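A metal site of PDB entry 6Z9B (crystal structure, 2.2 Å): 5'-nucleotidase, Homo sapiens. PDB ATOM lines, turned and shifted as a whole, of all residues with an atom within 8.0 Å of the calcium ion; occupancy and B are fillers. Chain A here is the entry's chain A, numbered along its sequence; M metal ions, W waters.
Water W2 bridges O of Gly 210 and NZ of Lys 183.
OD1 of Asp 270 is in hydrogen-bond range of N of Gly 273 (3.3 Å).
The side-chain amino group (NZ) of Lys 189 is in hydrogen-bond range of the side-chain amide oxygen (OD1) of Asn 188.
O of Ile 190 lies within hydrogen-bond range of N of Asp 212 (2.8 Å).
Of the 17 residues printed, 3 come within 4 Å of the calcium ion.
The calcium ion is bound by O of Asn 188, O of Gly 273, water W2, OD2 of Asp 212, OD1 of Asp 212 and water W1.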
ATOM      1  N   LYS A 183      23.415 -10.110 -15.820  1.00  0.00           N
ATOM      2  CA  LYS A 183      22.647 -10.232 -14.576  1.00  0.00           C
ATOM      3  C   LYS A 183      22.536 -11.700 -14.130  1.00  0.00           C
ATOM      4  O   LYS A 183      22.517 -11.954 -12.920  1.00  0.00           O
ATOM      5  CB  LYS A 183      21.244  -9.619 -14.749  1.00  0.00           C
ATOM      6  CG  LYS A 183      21.242  -8.090 -14.842  1.00  0.00           C
ATOM      7  CD  LYS A 183      21.048  -7.454 -13.474  1.00  0.00           C
ATOM      8  CE  LYS A 183      21.817  -6.164 -13.310  1.00  0.00           C
ATOM      9  NZ  LYS A 183      23.199  -6.375 -12.779  1.00  0.00           N
ATOM     10  N   VAL A 187      26.708 -10.463 -12.536  1.00  0.00           N
ATOM     11  CA  VAL A 187      27.521  -9.264 -12.693  1.00  0.00           C
ATOM     12  C   VAL A 187      26.590  -8.127 -12.270  1.00  0.00           C
ATOM     13  O   VAL A 187      25.561  -7.899 -12.903  1.00  0.00           O
ATOM     14  CB  VAL A 187      28.104  -9.096 -14.114  1.00  0.00           C
ATOM     15  CG1 VAL A 187      28.941  -7.825 -14.212  1.00  0.00           C
ATOM     16  CG2 VAL A 187      28.948 -10.316 -14.493  1.00  0.00           C
ATOM     17  N   ASN A 188      26.919  -7.470 -11.150  1.00  0.00           N
ATOM     18  CA  ASN A 188      26.056  -6.424 -10.602  1.00  0.00           C
ATOM     19  C   ASN A 188      26.491  -4.992 -10.914  1.00  0.00           C
ATOM     20  O   ASN A 188      25.789  -4.069 -10.514  1.00  0.00           O
ATOM     21  CB  ASN A 188      25.877  -6.618  -9.086  1.00  0.00           C
ATOM     22  CG  ASN A 188      27.164  -6.613  -8.307  1.00  0.00           C
ATOM     23  OD1 ASN A 188      28.162  -5.959  -8.671  1.00  0.00           O
ATOM     24  ND2 ASN A 188      27.158  -7.324  -7.198  1.00  0.00           N
ATOM     25  N   LYS A 189      27.631  -4.809 -11.617  1.00  0.00           N
ATOM     26  CA  LYS A 189      28.148  -3.500 -11.992  1.00  0.00           C
ATOM     27  C   LYS A 189      28.203  -3.470 -13.515  1.00  0.00           C
ATOM     28  O   LYS A 189      28.899  -4.291 -14.119  1.00  0.00           O
ATOM     29  CB  LYS A 189      29.503  -3.203 -11.313  1.00  0.00           C
ATOM     30  CG  LYS A 189      29.353  -2.984  -9.818  1.00  0.00           C
ATOM     31  CD  LYS A 189      30.698  -2.804  -9.054  1.00  0.00           C
ATOM     32  CE  LYS A 189      31.441  -4.069  -8.682  1.00  0.00           C
ATOM     33  NZ  LYS A 189      30.654  -4.924  -7.772  1.00  0.00           N
ATOM     34  N   ILE A 190      27.360  -2.623 -14.155  1.00  0.00           N
ATOM     35  CA  ILE A 190      27.219  -2.612 -15.621  1.00  0.00           C
ATOM     36  C   ILE A 190      27.325  -1.201 -16.222  1.00  0.00           C
ATOM     37  O   ILE A 190      26.560  -0.314 -15.845  1.00  0.00           O
ATOM     38  CB  ILE A 190      25.913  -3.388 -16.080  1.00  0.00           C
ATOM     39  CG1 ILE A 190      25.931  -4.868 -15.579  1.00  0.00           C
ATOM     40  CG2 ILE A 190      25.719  -3.332 -17.648  1.00  0.00           C
ATOM     41  CD1 ILE A 190      24.700  -5.682 -15.775  1.00  0.00           C
ATOM     42  N   ILE A 191      28.265  -1.040 -17.172  1.00  0.00           N
ATOM     43  CA  ILE A 191      28.520   0.175 -17.929  1.00  0.00           C
ATOM     44  C   ILE A 191      28.012  -0.048 -19.346  1.00  0.00           C
ATOM     45  O   ILE A 191      28.390  -1.048 -19.949  1.00  0.00           O
ATOM     46  CB  ILE A 191      30.055   0.509 -17.977  1.00  0.00           C
ATOM     47  CG1 ILE A 191      30.686   0.666 -16.564  1.00  0.00           C
ATOM     48  CG2 ILE A 191      30.356   1.759 -18.867  1.00  0.00           C
ATOM     49  CD1 ILE A 191      32.221   0.617 -16.582  1.00  0.00           C
ATOM     50  N   GLY A 210      19.123  -2.240 -15.625  1.00  0.00           N
ATOM     51  CA  GLY A 210      20.372  -2.868 -15.211  1.00  0.00           C
ATOM     52  C   GLY A 210      21.634  -2.104 -15.549  1.00  0.00           C
ATOM     53  O   GLY A 210      22.693  -2.457 -15.038  1.00  0.00           O
ATOM     54  N   VAL A 211      21.556  -1.083 -16.424  1.00  0.00           N
ATOM     55  CA  VAL A 211      22.719  -0.263 -16.769  1.00  0.00           C
ATOM     56  C   VAL A 211      22.929   0.769 -15.620  1.00  0.00           C
ATOM     57  O   VAL A 211      21.984   1.478 -15.231  1.00  0.00           O
ATOM     58  CB  VAL A 211      22.574   0.418 -18.165  1.00  0.00           C
ATOM     59  CG1 VAL A 211      23.608   1.516 -18.364  1.00  0.00           C
ATOM     60  CG2 VAL A 211      22.645  -0.612 -19.302  1.00  0.00           C
ATOM     61  N   ASP A 212      24.137   0.820 -15.070  1.00  0.00           N
ATOM     62  CA  ASP A 212      24.501   1.732 -13.987  1.00  0.00           C
ATOM     63  C   ASP A 212      25.079   3.035 -14.478  1.00  0.00           C
ATOM     64  O   ASP A 212      24.895   4.048 -13.805  1.00  0.00           O
ATOM     65  CB  ASP A 212      25.511   1.070 -13.022  1.00  0.00           C
ATOM     66  CG  ASP A 212      24.969  -0.159 -12.352  1.00  0.00           C
ATOM     67  OD1 ASP A 212      23.819  -0.094 -11.846  1.00  0.00           O
ATOM     68  OD2 ASP A 212      25.682  -1.190 -12.332  1.00  0.00           O
ATOM     69  N   VAL A 213      25.851   2.990 -15.587  1.00  0.00           N
ATOM     70  CA  VAL A 213      26.530   4.158 -16.165  1.00  0.00           C
ATOM     71  C   VAL A 213      26.420   4.074 -17.677  1.00  0.00           C
ATOM     72  O   VAL A 213      26.581   2.992 -18.235  1.00  0.00           O
ATOM     73  CB  VAL A 213      28.039   4.237 -15.834  1.00  0.00           C
ATOM     74  CG1 VAL A 213      28.537   5.667 -15.840  1.00  0.00           C
ATOM     75  CG2 VAL A 213      28.423   3.509 -14.570  1.00  0.00           C
ATOM     76  N   ARG A 248      15.978   4.521 -10.827  1.00  0.00           N
ATOM     77  CA  ARG A 248      17.380   4.708 -10.445  1.00  0.00           C
ATOM     78  C   ARG A 248      18.006   5.900 -11.155  1.00  0.00           C
ATOM     79  O   ARG A 248      17.816   6.078 -12.356  1.00  0.00           O
ATOM     80  CB  ARG A 248      18.231   3.467 -10.764  1.00  0.00           C
ATOM     81  CG  ARG A 248      17.740   2.106 -10.212  1.00  0.00           C
ATOM     82  CD  ARG A 248      18.559   0.932 -10.760  1.00  0.00           C
ATOM     83  NE  ARG A 248      18.337   0.733 -12.200  1.00  0.00           N
ATOM     84  CZ  ARG A 248      19.144   1.181 -13.168  1.00  0.00           C
ATOM     85  NH1 ARG A 248      18.837   0.983 -14.440  1.00  0.00           N
ATOM     86  NH2 ARG A 248      20.254   1.845 -12.863  1.00  0.00           N
ATOM     87  N   PHE A 269      30.005   2.488  -5.504  1.00  0.00           N
ATOM     88  CA  PHE A 269      29.000   1.430  -5.602  1.00  0.00           C
ATOM     89  C   PHE A 269      28.825   0.791  -4.216  1.00  0.00           C
ATOM     90  O   PHE A 269      29.745   0.836  -3.391  1.00  0.00           O
ATOM     91  CB  PHE A 269      29.451   0.334  -6.586  1.00  0.00           C
ATOM     92  CG  PHE A 269      29.457   0.647  -8.074  1.00  0.00           C
ATOM     93  CD1 PHE A 269      28.295   0.525  -8.834  1.00  0.00           C
ATOM     94  CD2 PHE A 269      30.647   0.920  -8.731  1.00  0.00           C
ATOM     95  CE1 PHE A 269      28.313   0.741 -10.208  1.00  0.00           C
ATOM     96  CE2 PHE A 269      30.662   1.119 -10.119  1.00  0.00           C
ATOM     97  CZ  PHE A 269      29.490   1.032 -10.835  1.00  0.00           C
ATOM     98  N   ASP A 270      27.665   0.159  -3.961  1.00  0.00           N
ATOM     99  CA  ASP A 270      27.540  -0.592  -2.716  1.00  0.00           C
ATOM    100  C   ASP A 270      27.889  -2.056  -3.054  1.00  0.00           C
ATOM    101  O   ASP A 270      28.300  -2.332  -4.203  1.00  0.00           O
ATOM    102  CB  ASP A 270      26.176  -0.381  -1.997  1.00  0.00           C
ATOM    103  CG  ASP A 270      24.923  -0.976  -2.611  1.00  0.00           C
ATOM    104  OD1 ASP A 270      25.031  -1.936  -3.389  1.00  0.00           O
ATOM    105  OD2 ASP A 270      23.809  -0.516  -2.246  1.00  0.00           O
ATOM    106  N   ARG A 272      25.992  -4.624  -3.543  1.00  0.00           N
ATOM    107  CA  ARG A 272      25.060  -5.190  -4.535  1.00  0.00           C
ATOM    108  C   ARG A 272      25.104  -4.494  -5.898  1.00  0.00           C
ATOM    109  O   ARG A 272      24.249  -4.758  -6.759  1.00  0.00           O
ATOM    110  CB  ARG A 272      23.632  -5.235  -3.962  1.00  0.00           C
ATOM    111  CG  ARG A 272      23.451  -6.234  -2.803  1.00  0.00           C
ATOM    112  CD  ARG A 272      23.161  -7.635  -3.309  1.00  0.00           C
ATOM    113  NE  ARG A 272      22.963  -8.567  -2.198  1.00  0.00           N
ATOM    114  CZ  ARG A 272      21.815  -9.142  -1.896  1.00  0.00           C
ATOM    115  NH1 ARG A 272      20.724  -8.901  -2.618  1.00  0.00           N
ATOM    116  NH2 ARG A 272      21.734  -9.987  -0.868  1.00  0.00           N
ATOM    117  N   GLY A 273      26.083  -3.611  -6.091  1.00  0.00           N
ATOM    118  CA  GLY A 273      26.287  -2.889  -7.343  1.00  0.00           C
ATOM    119  C   GLY A 273      25.367  -1.701  -7.564  1.00  0.00           C
ATOM    120  O   GLY A 273      25.311  -1.162  -8.694  1.00  0.00           O
ATOM    121  N   ASN A 274      24.641  -1.279  -6.507  1.00  0.00           N
ATOM    122  CA  ASN A 274      23.770  -0.099  -6.595  1.00  0.00           C
ATOM    123  C   ASN A 274      24.681   1.132  -6.602  1.00  0.00           C
ATOM    124  O   ASN A 274      25.656   1.156  -5.867  1.00  0.00           O
ATOM    125  CB  ASN A 274      22.849  -0.009  -5.366  1.00  0.00           C
ATOM    126  CG  ASN A 274      21.848  -1.116  -5.190  1.00  0.00           C
ATOM    127  OD1 ASN A 274      21.850  -1.834  -4.181  1.00  0.00           O
ATOM    128  ND2 ASN A 274      20.942  -1.275  -6.154  1.00  0.00           N
ATOM    129  N   VAL A 275      24.389   2.127  -7.450  1.00  0.00           N
ATOM    130  CA  VAL A 275      25.189   3.350  -7.506  1.00  0.00           C
ATOM    131  C   VAL A 275      24.742   4.185  -6.324  1.00  0.00           C
ATOM    132  O   VAL A 275      23.560   4.473  -6.191  1.00  0.00           O
ATOM    133  CB  VAL A 275      25.060   4.135  -8.840  1.00  0.00           C
ATOM    134  CG1 VAL A 275      25.739   5.496  -8.752  1.00  0.00           C
ATOM    135  CG2 VAL A 275      25.641   3.340 -10.002  1.00  0.00           C
HETATM  136 CA    CA M   1      24.308  -2.314 -10.509  1.00  0.00          CA
HETATM  137  O   HOH W   1      22.162  -3.384  -9.073  1.00  0.00           O
HETATM  138  O   HOH W   2      23.146  -3.418 -12.451  1.00  0.00           O
